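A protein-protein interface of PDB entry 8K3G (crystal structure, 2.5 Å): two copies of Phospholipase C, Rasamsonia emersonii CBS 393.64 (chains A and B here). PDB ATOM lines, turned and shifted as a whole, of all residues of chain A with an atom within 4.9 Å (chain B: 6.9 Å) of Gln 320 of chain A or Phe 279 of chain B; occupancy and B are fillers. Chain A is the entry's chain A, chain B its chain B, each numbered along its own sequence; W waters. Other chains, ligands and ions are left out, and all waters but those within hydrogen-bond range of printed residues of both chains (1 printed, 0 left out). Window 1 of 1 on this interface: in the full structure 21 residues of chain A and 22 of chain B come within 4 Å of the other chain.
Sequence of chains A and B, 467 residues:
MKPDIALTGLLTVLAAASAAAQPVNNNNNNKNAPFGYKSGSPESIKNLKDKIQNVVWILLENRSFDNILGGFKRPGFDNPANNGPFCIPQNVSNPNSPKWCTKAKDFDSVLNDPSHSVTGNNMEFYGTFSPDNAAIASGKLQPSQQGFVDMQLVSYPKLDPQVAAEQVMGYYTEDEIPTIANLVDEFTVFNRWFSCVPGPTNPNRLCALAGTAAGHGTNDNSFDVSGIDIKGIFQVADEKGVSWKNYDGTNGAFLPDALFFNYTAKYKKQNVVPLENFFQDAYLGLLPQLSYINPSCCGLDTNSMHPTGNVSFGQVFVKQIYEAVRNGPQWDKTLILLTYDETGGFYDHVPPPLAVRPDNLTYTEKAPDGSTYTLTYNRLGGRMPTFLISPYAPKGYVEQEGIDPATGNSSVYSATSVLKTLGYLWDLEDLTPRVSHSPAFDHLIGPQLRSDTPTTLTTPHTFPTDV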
ATOM      1  N   GLU A 276      26.092  -3.414   3.463  1.00  0.00           N
ATOM      2  CA  GLU A 276      26.634  -2.966   4.746  1.00  0.00           C
ATOM      3  C   GLU A 276      27.635  -3.959   5.325  1.00  0.00           C
ATOM      4  O   GLU A 276      28.562  -3.558   6.048  1.00  0.00           O
ATOM      5  CB  GLU A 276      25.487  -2.751   5.742  1.00  0.00           C
ATOM      6  CG  GLU A 276      25.809  -2.225   7.175  1.00  0.00           C
ATOM      7  CD  GLU A 276      26.964  -1.217   7.303  1.00  0.00           C
ATOM      8  OE1 GLU A 276      27.198  -0.404   6.392  1.00  0.00           O
ATOM      9  OE2 GLU A 276      27.604  -1.192   8.375  1.00  0.00           O
ATOM     10  N   PHE A 279      31.374  -2.996   4.444  1.00  0.00           N
ATOM     11  CA  PHE A 279      32.069  -2.026   5.279  1.00  0.00           C
ATOM     12  C   PHE A 279      32.416  -2.646   6.619  1.00  0.00           C
ATOM     13  O   PHE A 279      33.519  -2.442   7.133  1.00  0.00           O
ATOM     14  CB  PHE A 279      31.210  -0.760   5.438  1.00  0.00           C
ATOM     15  CG  PHE A 279      30.735  -0.210   4.122  1.00  0.00           C
ATOM     16  CD1 PHE A 279      31.646   0.103   3.130  1.00  0.00           C
ATOM     17  CD2 PHE A 279      29.380  -0.073   3.850  1.00  0.00           C
ATOM     18  CE1 PHE A 279      31.229   0.569   1.900  1.00  0.00           C
ATOM     19  CE2 PHE A 279      28.944   0.397   2.626  1.00  0.00           C
ATOM     20  CZ  PHE A 279      29.871   0.718   1.643  1.00  0.00           C
ATOM     21  N   VAL A 316      30.558   8.700  -3.718  1.00  0.00           N
ATOM     22  CA  VAL A 316      30.430   8.415  -2.288  1.00  0.00           C
ATOM     23  C   VAL A 316      30.626   6.926  -2.046  1.00  0.00           C
ATOM     24  O   VAL A 316      31.404   6.505  -1.182  1.00  0.00           O
ATOM     25  CB  VAL A 316      29.069   8.904  -1.756  1.00  0.00           C
ATOM     26  CG1 VAL A 316      28.768   8.318  -0.345  1.00  0.00           C
ATOM     27  CG2 VAL A 316      29.037  10.404  -1.733  1.00  0.00           C
ATOM     28  N   PHE A 317      29.928   6.112  -2.840  1.00  0.00           N
ATOM     29  CA  PHE A 317      30.104   4.665  -2.852  1.00  0.00           C
ATOM     30  C   PHE A 317      31.578   4.274  -2.999  1.00  0.00           C
ATOM     31  O   PHE A 317      32.100   3.478  -2.208  1.00  0.00           O
ATOM     32  CB  PHE A 317      29.254   4.106  -3.995  1.00  0.00           C
ATOM     33  CG  PHE A 317      29.189   2.610  -4.065  1.00  0.00           C
ATOM     34  CD1 PHE A 317      28.678   1.862  -3.012  1.00  0.00           C
ATOM     35  CD2 PHE A 317      29.585   1.949  -5.227  1.00  0.00           C
ATOM     36  CE1 PHE A 317      28.582   0.474  -3.107  1.00  0.00           C
ATOM     37  CE2 PHE A 317      29.484   0.558  -5.324  1.00  0.00           C
ATOM     38  CZ  PHE A 317      28.984  -0.177  -4.255  1.00  0.00           C
ATOM     39  N   VAL A 318      32.271   4.837  -4.001  1.00  0.00           N
ATOM     40  CA  VAL A 318      33.682   4.501  -4.200  1.00  0.00           C
ATOM     41  C   VAL A 318      34.501   4.903  -2.979  1.00  0.00           C
ATOM     42  O   VAL A 318      35.379   4.156  -2.523  1.00  0.00           O
ATOM     43  CB  VAL A 318      34.212   5.151  -5.492  1.00  0.00           C
ATOM     44  CG1 VAL A 318      35.751   5.082  -5.560  1.00  0.00           C
ATOM     45  CG2 VAL A 318      33.577   4.492  -6.696  1.00  0.00           C
ATOM     46  N   LYS A 319      34.191   6.067  -2.401  1.00  0.00           N
ATOM     47  CA  LYS A 319      34.913   6.536  -1.223  1.00  0.00           C
ATOM     48  C   LYS A 319      34.687   5.603  -0.033  1.00  0.00           C
ATOM     49  O   LYS A 319      35.635   5.259   0.685  1.00  0.00           O
ATOM     50  CB  LYS A 319      34.478   7.975  -0.916  1.00  0.00           C
ATOM     51  CG  LYS A 319      34.905   8.534   0.416  1.00  0.00           C
ATOM     52  CD  LYS A 319      34.434   9.978   0.567  1.00  0.00           C
ATOM     53  CE  LYS A 319      34.523  10.453   2.034  1.00  0.00           C
ATOM     54  NZ  LYS A 319      35.895  10.910   2.431  1.00  0.00           N
ATOM     55  N   GLN A 320      33.441   5.160   0.172  1.00  0.00           N
ATOM     56  CA  GLN A 320      33.135   4.219   1.251  1.00  0.00           C
ATOM     57  C   GLN A 320      33.904   2.917   1.084  1.00  0.00           C
ATOM     58  O   GLN A 320      34.500   2.406   2.038  1.00  0.00           O
ATOM     59  CB  GLN A 320      31.640   3.912   1.283  1.00  0.00           C
ATOM     60  CG  GLN A 320      30.726   4.990   1.824  1.00  0.00           C
ATOM     61  CD  GLN A 320      29.280   4.538   1.737  1.00  0.00           C
ATOM     62  OE1 GLN A 320      28.732   4.004   2.705  1.00  0.00           O
ATOM     63  NE2 GLN A 320      28.665   4.716   0.562  1.00  0.00           N
ATOM     64  N   ILE A 321      33.862   2.343  -0.122  1.00  0.00           N
ATOM     65  CA  ILE A 321      34.546   1.085  -0.371  1.00  0.00           C
ATOM     66  C   ILE A 321      36.033   1.231  -0.066  1.00  0.00           C
ATOM     67  O   ILE A 321      36.609   0.444   0.698  1.00  0.00           O
ATOM     68  CB  ILE A 321      34.306   0.638  -1.819  1.00  0.00           C
ATOM     69  CG1 ILE A 321      32.836   0.295  -2.024  1.00  0.00           C
ATOM     70  CG2 ILE A 321      35.231  -0.502  -2.217  1.00  0.00           C
ATOM     71  CD1 ILE A 321      32.419   0.429  -3.483  1.00  0.00           C
ATOM     72  N   TYR A 322      36.663   2.270  -0.633  1.00  0.00           N
ATOM     73  CA  TYR A 322      38.098   2.479  -0.461  1.00  0.00           C
ATOM     74  C   TYR A 322      38.468   2.657   1.004  1.00  0.00           C
ATOM     75  O   TYR A 322      39.438   2.062   1.483  1.00  0.00           O
ATOM     76  CB  TYR A 322      38.572   3.704  -1.250  1.00  0.00           C
ATOM     77  CG  TYR A 322      40.018   4.053  -0.931  1.00  0.00           C
ATOM     78  CD1 TYR A 322      41.062   3.433  -1.608  1.00  0.00           C
ATOM     79  CD2 TYR A 322      40.340   4.979   0.062  1.00  0.00           C
ATOM     80  CE1 TYR A 322      42.373   3.738  -1.312  1.00  0.00           C
ATOM     81  CE2 TYR A 322      41.643   5.294   0.355  1.00  0.00           C
ATOM     82  CZ  TYR A 322      42.663   4.665  -0.329  1.00  0.00           C
ATOM     83  OH  TYR A 322      43.982   4.960  -0.042  1.00  0.00           O
ATOM     84  N   GLU A 323      37.733   3.512   1.723  1.00  0.00           N
ATOM     85  CA  GLU A 323      38.135   3.833   3.087  1.00  0.00           C
ATOM     86  C   GLU A 323      37.964   2.641   4.018  1.00  0.00           C
ATOM     87  O   GLU A 323      38.778   2.456   4.930  1.00  0.00           O
ATOM     88  CB  GLU A 323      37.370   5.067   3.580  1.00  0.00           C
ATOM     89  CG  GLU A 323      37.905   6.317   2.854  1.00  0.00           C
ATOM     90  CD  GLU A 323      37.172   7.599   3.182  1.00  0.00           C
ATOM     91  OE1 GLU A 323      36.270   7.585   4.045  1.00  0.00           O
ATOM     92  OE2 GLU A 323      37.509   8.636   2.571  1.00  0.00           O
ATOM     93  N   ALA A 324      36.949   1.802   3.780  1.00  0.00           N
ATOM     94  CA  ALA A 324      36.752   0.618   4.613  1.00  0.00           C
ATOM     95  C   ALA A 324      37.897  -0.381   4.436  1.00  0.00           C
ATOM     96  O   ALA A 324      38.418  -0.919   5.422  1.00  0.00           O
ATOM     97  CB  ALA A 324      35.402  -0.028   4.297  1.00  0.00           C
ATOM     98  N   TYR B 247      16.030   5.560   8.029  1.00  0.00           N
ATOM     99  CA  TYR B 247      17.009   4.806   7.259  1.00  0.00           C
ATOM    100  C   TYR B 247      17.054   3.373   7.790  1.00  0.00           C
ATOM    101  O   TYR B 247      17.357   3.144   8.974  1.00  0.00           O
ATOM    102  CB  TYR B 247      18.379   5.480   7.329  1.00  0.00           C
ATOM    103  CG  TYR B 247      18.404   6.833   6.671  1.00  0.00           C
ATOM    104  CD1 TYR B 247      18.638   6.956   5.303  1.00  0.00           C
ATOM    105  CD2 TYR B 247      18.186   7.999   7.409  1.00  0.00           C
ATOM    106  CE1 TYR B 247      18.661   8.208   4.677  1.00  0.00           C
ATOM    107  CE2 TYR B 247      18.214   9.261   6.793  1.00  0.00           C
ATOM    108  CZ  TYR B 247      18.454   9.349   5.429  1.00  0.00           C
ATOM    109  OH  TYR B 247      18.488  10.570   4.816  1.00  0.00           O
ATOM    110  N   PRO B 274      16.750   2.602   2.235  1.00  0.00           N
ATOM    111  CA  PRO B 274      17.835   1.716   2.690  1.00  0.00           C
ATOM    112  C   PRO B 274      18.907   2.453   3.479  1.00  0.00           C
ATOM    113  O   PRO B 274      19.095   3.665   3.371  1.00  0.00           O
ATOM    114  CB  PRO B 274      18.420   1.143   1.387  1.00  0.00           C
ATOM    115  CG  PRO B 274      17.367   1.373   0.347  1.00  0.00           C
ATOM    116  CD  PRO B 274      16.631   2.616   0.764  1.00  0.00           C
ATOM    117  N   LEU B 275      19.623   1.675   4.287  1.00  0.00           N
ATOM    118  CA  LEU B 275      20.694   2.221   5.110  1.00  0.00           C
ATOM    119  C   LEU B 275      21.721   2.989   4.281  1.00  0.00           C
ATOM    120  O   LEU B 275      22.244   4.018   4.731  1.00  0.00           O
ATOM    121  CB  LEU B 275      21.377   1.091   5.885  1.00  0.00           C
ATOM    122  CG  LEU B 275      22.530   1.550   6.788  1.00  0.00           C
ATOM    123  CD1 LEU B 275      22.062   2.676   7.730  1.00  0.00           C
ATOM    124  CD2 LEU B 275      23.220   0.364   7.550  1.00  0.00           C
ATOM    125  N   GLU B 276      22.059   2.487   3.086  1.00  0.00           N
ATOM    126  CA  GLU B 276      23.119   3.127   2.310  1.00  0.00           C
ATOM    127  C   GLU B 276      22.738   4.548   1.918  1.00  0.00           C
ATOM    128  O   GLU B 276      23.620   5.408   1.778  1.00  0.00           O
ATOM    129  CB  GLU B 276      23.452   2.292   1.066  1.00  0.00           C
ATOM    130  CG  GLU B 276      24.365   2.966   0.025  1.00  0.00           C
ATOM    131  CD  GLU B 276      25.807   3.227   0.505  1.00  0.00           C
ATOM    132  OE1 GLU B 276      26.191   2.742   1.596  1.00  0.00           O
ATOM    133  OE2 GLU B 276      26.567   3.927  -0.222  1.00  0.00           O
ATOM    134  N   ASN B 277      21.430   4.808   1.756  1.00  0.00           N
ATOM    135  CA  ASN B 277      20.947   6.162   1.493  1.00  0.00           C
ATOM    136  C   ASN B 277      21.414   7.143   2.564  1.00  0.00           C
ATOM    137  O   ASN B 277      21.603   8.330   2.272  1.00  0.00           O
ATOM    138  CB  ASN B 277      19.409   6.198   1.393  1.00  0.00           C
ATOM    139  CG  ASN B 277      18.874   5.444   0.181  1.00  0.00           C
ATOM    140  OD1 ASN B 277      19.393   4.389  -0.171  1.00  0.00           O
ATOM    141  ND2 ASN B 277      17.852   5.992  -0.476  1.00  0.00           N
ATOM    142  N   PHE B 278      21.600   6.687   3.808  1.00  0.00           N
ATOM    143  CA  PHE B 278      22.030   7.633   4.826  1.00  0.00           C
ATOM    144  C   PHE B 278      23.445   8.121   4.547  1.00  0.00           C
ATOM    145  O   PHE B 278      23.704   9.330   4.534  1.00  0.00           O
ATOM    146  CB  PHE B 278      21.944   7.039   6.228  1.00  0.00           C
ATOM    147  CG  PHE B 278      22.443   7.981   7.270  1.00  0.00           C
ATOM    148  CD1 PHE B 278      21.605   8.947   7.790  1.00  0.00           C
ATOM    149  CD2 PHE B 278      23.772   7.963   7.665  1.00  0.00           C
ATOM    150  CE1 PHE B 278      22.070   9.858   8.724  1.00  0.00           C
ATOM    151  CE2 PHE B 278      24.249   8.867   8.595  1.00  0.00           C
ATOM    152  CZ  PHE B 278      23.390   9.824   9.128  1.00  0.00           C
ATOM    153  N   PHE B 279      24.370   7.191   4.307  1.00  0.00           N
ATOM    154  CA  PHE B 279      25.744   7.577   4.011  1.00  0.00           C
ATOM    155  C   PHE B 279      25.803   8.507   2.799  1.00  0.00           C
ATOM    156  O   PHE B 279      26.483   9.539   2.826  1.00  0.00           O
ATOM    157  CB  PHE B 279      26.596   6.310   3.828  1.00  0.00           C
ATOM    158  CG  PHE B 279      26.518   5.367   5.021  1.00  0.00           C
ATOM    159  CD1 PHE B 279      26.724   5.852   6.313  1.00  0.00           C
ATOM    160  CD2 PHE B 279      26.184   4.022   4.861  1.00  0.00           C
ATOM    161  CE1 PHE B 279      26.622   5.028   7.409  1.00  0.00           C
ATOM    162  CE2 PHE B 279      26.084   3.178   5.966  1.00  0.00           C
ATOM    163  CZ  PHE B 279      26.298   3.682   7.241  1.00  0.00           C
ATOM    164  N   GLN B 280      25.070   8.170   1.737  1.00  0.00           N
ATOM    165  CA  GLN B 280      24.957   9.052   0.579  1.00  0.00           C
ATOM    166  C   GLN B 280      24.466  10.440   0.988  1.00  0.00           C
ATOM    167  O   GLN B 280      25.109  11.452   0.678  1.00  0.00           O
ATOM    168  CB  GLN B 280      24.021   8.420  -0.471  1.00  0.00           C
ATOM    169  CG  GLN B 280      24.601   7.145  -1.126  1.00  0.00           C
ATOM    170  CD  GLN B 280      23.560   6.339  -1.885  1.00  0.00           C
ATOM    171  OE1 GLN B 280      22.373   6.668  -1.849  1.00  0.00           O
ATOM    172  NE2 GLN B 280      23.990   5.261  -2.551  1.00  0.00           N
ATOM    173  N   ASP B 281      23.340  10.502   1.717  1.00  0.00           N
ATOM    174  CA  ASP B 281      22.750  11.790   2.064  1.00  0.00           C
ATOM    175  C   ASP B 281      23.666  12.598   2.982  1.00  0.00           C
ATOM    176  O   ASP B 281      23.848  13.805   2.776  1.00  0.00           O
ATOM    177  CB  ASP B 281      21.386  11.591   2.714  1.00  0.00           C
ATOM    178  CG  ASP B 281      20.331  11.114   1.726  1.00  0.00           C
ATOM    179  OD1 ASP B 281      20.625  11.071   0.508  1.00  0.00           O
ATOM    180  OD2 ASP B 281      19.206  10.784   2.170  1.00  0.00           O
ATOM    181  N   ALA B 282      24.284  11.946   3.975  1.00  0.00           N
ATOM    182  CA  ALA B 282      25.088  12.686   4.940  1.00  0.00           C
ATOM    183  C   ALA B 282      26.370  13.227   4.305  1.00  0.00           C
ATOM    184  O   ALA B 282      26.743  14.381   4.546  1.00  0.00           O
ATOM    185  CB  ALA B 282      25.386  11.810   6.162  1.00  0.00           C
ATOM    186  N   TYR B 283      27.056  12.428   3.487  1.00  0.00           N
ATOM    187  CA  TYR B 283      28.267  12.938   2.828  1.00  0.00           C
ATOM    188  C   TYR B 283      27.948  14.055   1.838  1.00  0.00           C
ATOM    189  O   TYR B 283      28.772  14.944   1.609  1.00  0.00           O
ATOM    190  CB  TYR B 283      28.998  11.820   2.084  1.00  0.00           C
ATOM    191  CG  TYR B 283      29.933  11.003   2.935  1.00  0.00           C
ATOM    192  CD1 TYR B 283      31.026  11.587   3.562  1.00  0.00           C
ATOM    193  CD2 TYR B 283      29.724   9.636   3.107  1.00  0.00           C
ATOM    194  CE1 TYR B 283      31.885  10.839   4.340  1.00  0.00           C
ATOM    195  CE2 TYR B 283      30.582   8.872   3.880  1.00  0.00           C
ATOM    196  CZ  TYR B 283      31.655   9.479   4.494  1.00  0.00           C
ATOM    197  OH  TYR B 283      32.494   8.714   5.263  1.00  0.00           O
ATOM    198  N   LEU B 284      26.772  14.017   1.230  1.00  0.00           N
ATOM    199  CA  LEU B 284      26.417  14.976   0.206  1.00  0.00           C
ATOM    200  C   LEU B 284      25.624  16.157   0.757  1.00  0.00           C
ATOM    201  O   LEU B 284      25.352  17.102   0.018  1.00  0.00           O
ATOM    202  CB  LEU B 284      25.642  14.256  -0.895  1.00  0.00           C
ATOM    203  CG  LEU B 284      26.408  13.816  -2.152  1.00  0.00           C
ATOM    204  CD1 LEU B 284      27.945  13.964  -2.059  1.00  0.00           C
ATOM    205  CD2 LEU B 284      25.994  12.422  -2.564  1.00  0.00           C
ATOM    206  N   GLY B 285      25.283  16.148   2.044  1.00  0.00           N
ATOM    207  CA  GLY B 285      24.489  17.225   2.603  1.00  0.00           C
ATOM    208  C   GLY B 285      23.051  17.222   2.151  1.00  0.00           C
ATOM    209  O   GLY B 285      22.471  18.289   1.970  1.00  0.00           O
ATOM    210  N   LEU B 287      20.631  15.381   3.923  1.00  0.00           N
ATOM    211  CA  LEU B 287      19.863  14.771   5.003  1.00  0.00           C
ATOM    212  C   LEU B 287      18.559  15.537   5.210  1.00  0.00           C
ATOM    213  O   LEU B 287      18.518  16.755   5.033  1.00  0.00           O
ATOM    214  CB  LEU B 287      20.658  14.753   6.312  1.00  0.00           C
ATOM    215  CG  LEU B 287      21.904  13.875   6.333  1.00  0.00           C
ATOM    216  CD1 LEU B 287      22.794  14.230   7.521  1.00  0.00           C
ATOM    217  CD2 LEU B 287      21.500  12.404   6.359  1.00  0.00           C
ATOM    218  N   ILE B 293      17.694   6.182  12.256  1.00  0.00           N
ATOM    219  CA  ILE B 293      18.442   5.056  11.692  1.00  0.00           C
ATOM    220  C   ILE B 293      18.146   3.797  12.500  1.00  0.00           C
ATOM    221  O   ILE B 293      18.402   3.758  13.709  1.00  0.00           O
ATOM    222  CB  ILE B 293      19.957   5.332  11.667  1.00  0.00           C
ATOM    223  CG1 ILE B 293      20.267   6.698  11.022  1.00  0.00           C
ATOM    224  CG2 ILE B 293      20.685   4.173  10.989  1.00  0.00           C
ATOM    225  CD1 ILE B 293      21.766   6.995  10.808  1.00  0.00           C
ATOM    226  N   VAL B 316      31.771  -0.146  14.144  1.00  0.00           N
ATOM    227  CA  VAL B 316      32.018   0.359  12.790  1.00  0.00           C
ATOM    228  C   VAL B 316      30.769   1.054  12.251  1.00  0.00           C
ATOM    229  O   VAL B 316      30.857   2.115  11.629  1.00  0.00           O
ATOM    230  CB  VAL B 316      32.558  -0.729  11.828  1.00  0.00           C
ATOM    231  CG1 VAL B 316      32.681  -2.045  12.480  1.00  0.00           C
ATOM    232  CG2 VAL B 316      31.775  -0.794  10.512  1.00  0.00           C
ATOM    233  N   PHE B 317      29.593   0.510  12.548  1.00  0.00           N
ATOM    234  CA  PHE B 317      28.332   1.185  12.254  1.00  0.00           C
ATOM    235  C   PHE B 317      28.328   2.623  12.777  1.00  0.00           C
ATOM    236  O   PHE B 317      28.050   3.574  12.035  1.00  0.00           O
ATOM    237  CB  PHE B 317      27.202   0.364  12.879  1.00  0.00           C
ATOM    238  CG  PHE B 317      25.832   0.871  12.588  1.00  0.00           C
ATOM    239  CD1 PHE B 317      25.404   1.060  11.282  1.00  0.00           C
ATOM    240  CD2 PHE B 317      24.946   1.133  13.633  1.00  0.00           C
ATOM    241  CE1 PHE B 317      24.116   1.524  11.016  1.00  0.00           C
ATOM    242  CE2 PHE B 317      23.658   1.589  13.382  1.00  0.00           C
ATOM    243  CZ  PHE B 317      23.236   1.777  12.067  1.00  0.00           C
ATOM    244  N   LYS B 319      30.956   4.421  13.717  1.00  0.00           N
ATOM    245  CA  LYS B 319      31.997   5.157  13.002  1.00  0.00           C
ATOM    246  C   LYS B 319      31.512   5.627  11.633  1.00  0.00           C
ATOM    247  O   LYS B 319      31.740   6.781  11.246  1.00  0.00           O
ATOM    248  CB  LYS B 319      33.235   4.274  12.866  1.00  0.00           C
ATOM    249  CG  LYS B 319      34.359   4.834  12.029  1.00  0.00           C
ATOM    250  CD  LYS B 319      35.515   3.837  11.992  1.00  0.00           C
ATOM    251  CE  LYS B 319      36.433   4.054  10.800  1.00  0.00           C
ATOM    252  NZ  LYS B 319      37.482   5.106  11.045  1.00  0.00           N
ATOM    253  N   GLN B 320      30.840   4.747  10.886  1.00  0.00           N
ATOM    254  CA  GLN B 320      30.314   5.115   9.573  1.00  0.00           C
ATOM    255  C   GLN B 320      29.338   6.287   9.663  1.00  0.00           C
ATOM    256  O   GLN B 320      29.435   7.253   8.898  1.00  0.00           O
ATOM    257  CB  GLN B 320      29.614   3.914   8.939  1.00  0.00           C
ATOM    258  CG  GLN B 320      30.487   2.812   8.382  1.00  0.00           C
ATOM    259  CD  GLN B 320      29.621   1.635   8.009  1.00  0.00           C
ATOM    260  OE1 GLN B 320      29.245   0.841   8.874  1.00  0.00           O
ATOM    261  NE2 GLN B 320      29.249   1.537   6.733  1.00  0.00           N
ATOM    262  N   ILE B 321      28.378   6.209  10.586  1.00  0.00           N
ATOM    263  CA  ILE B 321      27.378   7.263  10.715  1.00  0.00           C
ATOM    264  C   ILE B 321      28.049   8.592  11.046  1.00  0.00           C
ATOM    265  O   ILE B 321      27.772   9.624  10.415  1.00  0.00           O
ATOM    266  CB  ILE B 321      26.325   6.875  11.774  1.00  0.00           C
ATOM    267  CG1 ILE B 321      25.560   5.622  11.325  1.00  0.00           C
ATOM    268  CG2 ILE B 321      25.374   8.055  12.076  1.00  0.00           C
ATOM    269  CD1 ILE B 321      24.703   4.978  12.402  1.00  0.00           C
ATOM    270  N   TYR B 322      28.959   8.584  12.025  1.00  0.00           N
ATOM    271  CA  TYR B 322      29.624   9.822  12.414  1.00  0.00           C
ATOM    272  C   TYR B 322      30.400  10.407  11.247  1.00  0.00           C
ATOM    273  O   TYR B 322      30.239  11.580  10.905  1.00  0.00           O
ATOM    274  CB  TYR B 322      30.554   9.591  13.608  1.00  0.00           C
ATOM    275  CG  TYR B 322      31.344  10.842  13.985  1.00  0.00           C
ATOM    276  CD1 TYR B 322      30.794  11.812  14.822  1.00  0.00           C
ATOM    277  CD2 TYR B 322      32.637  11.061  13.487  1.00  0.00           C
ATOM    278  CE1 TYR B 322      31.510  12.968  15.159  1.00  0.00           C
ATOM    279  CE2 TYR B 322      33.360  12.210  13.825  1.00  0.00           C
ATOM    280  CZ  TYR B 322      32.788  13.156  14.659  1.00  0.00           C
ATOM    281  OH  TYR B 322      33.490  14.287  14.988  1.00  0.00           O
ATOM    282  N   ALA B 324      30.178  10.017   8.041  1.00  0.00           N
ATOM    283  CA  ALA B 324      29.376  10.519   6.929  1.00  0.00           C
ATOM    284  C   ALA B 324      28.817  11.908   7.236  1.00  0.00           C
ATOM    285  O   ALA B 324      28.828  12.804   6.376  1.00  0.00           O
ATOM    286  CB  ALA B 324      28.252   9.533   6.616  1.00  0.00           C
ATOM    287  N   VAL B 325      28.312  12.105   8.452  1.00  0.00           N
ATOM    288  CA  VAL B 325      27.767  13.407   8.813  1.00  0.00           C
ATOM    289  C   VAL B 325      28.903  14.410   8.999  1.00  0.00           C
ATOM    290  O   VAL B 325      28.869  15.529   8.471  1.00  0.00           O
ATOM    291  CB  VAL B 325      26.891  13.283  10.076  1.00  0.00           C
ATOM    292  CG1 VAL B 325      26.423  14.659  10.548  1.00  0.00           C
ATOM    293  CG2 VAL B 325      25.690  12.343   9.815  1.00  0.00           C
HETATM  294  O   HOH W   1      33.903   6.472   4.465  1.00  0.00           O
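The side-chain amide oxygen of Gln 320 of chain A lies close to the side-chain carboxylate of Glu 276 of chain B, 3.0 Å away. OE1 of Gln 320 of chain B sits close to OE2 of Glu 276 of chain A (2.7 Å).
The side-chain amino group (NZ) of Lys 319 of chain A lies within salt-bridge range of the side-chain carboxylate (OE2) of Glu 323 of chain A (2.8 Å). OE1 of Gln 320 of chain B lies close to O of Val 316 of chain B, 3.4 Å away. O of Ala 324 of chain B sits at hydrogen-bond distance from N of Tyr 283 of chain B (3.4 Å).
Among the printed residues, pairs that only touch across the chains: Glu 276 of chain A with Leu 275 of chain B (3.7 Å), Glu 276 of chain A with Phe 279 of chain B (3.8 Å), Phe 279 of chain A with Glu 276 of chain B (3.8 Å), Phe 279 of chain A with Gln 320 of chain B (3.3 Å), Val 316 of chain A with Gln 280 of chain B (3.99 Å), Val 316 of chain A with Tyr 283 of chain B (3.8 Å), Val 316 of chain A with Leu 284 of chain B (3.7 Å), Lys 319 of chain A with Tyr 283 of chain B (3.5 Å) and Gln 320 of chain A with Phe 279 of chain B (3.3 Å).
Of the printed residues of chain B, Phe 279 of chain A touches Glu 276 (3.8 Å) and Gln 320 (3.3 Å). Val 318 of chain A touches none of the printed residues of chain B. Gln 320 of chain A touches just these residues of chain B: Glu 276 and Phe 279. Printed residues of chain A within 4 Å of Glu 276 of chain B: Phe 279 and Gln 320. Phe 279 of chain B touches just these residues of chain A: Glu 276 and Gln 320. Printed residues of chain A within 4 Å of Tyr 283 of chain B: Val 316 and Lys 319. Ile 293 of chain B touches none of the printed residues of chain A. The nearest residue of chain B that does not touch Gln 320 of chain A is Tyr 283 of chain B (4.4 Å).
Of the 11 printed residues of chain A, 5 touch a printed residue of chain B. Hydrophobic or aromatic side chains of chain A within 4 Å of the printed part of chain B: Phe 279 and Val 316. Of the 23 printed residues of chain B, 7 touch a printed residue of chain A. Hydrophobic or aromatic side chains of chain B that line the printed part of chain A: Leu 275, Phe 279, Tyr 283 and Leu 284. Among the printed residues, 11 pairs touch across the chains. Among the printed residues, no Asp or Glu carboxylate lies within 4 Å of a Lys or Arg side-chain nitrogen of the other chain.
Glu 276 of chain A touches Phe 279 of chain B, and with the chains exchanged Phe 279 of chain A touches Glu 276 of chain B. Glu 276 of chain A touches Gln 320 of chain B, and with the chains exchanged Gln 320 of chain A touches Glu 276 of chain B. Phe 279 of chain A touches Gln 320 of chain B, and with the chains exchanged Gln 320 of chain A touches Phe 279 of chain B. 9 positions are printed for both chains. Of the 11 pairs that touch across the chains among the printed residues, 6 have their exchanged pair printed and touching as well.
Water W1 bridges the side-chain carboxylate of Glu 323 of chain A (2.6 Å) and the side-chain hydroxyl of Tyr 283 of chain B (2.8 Å).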
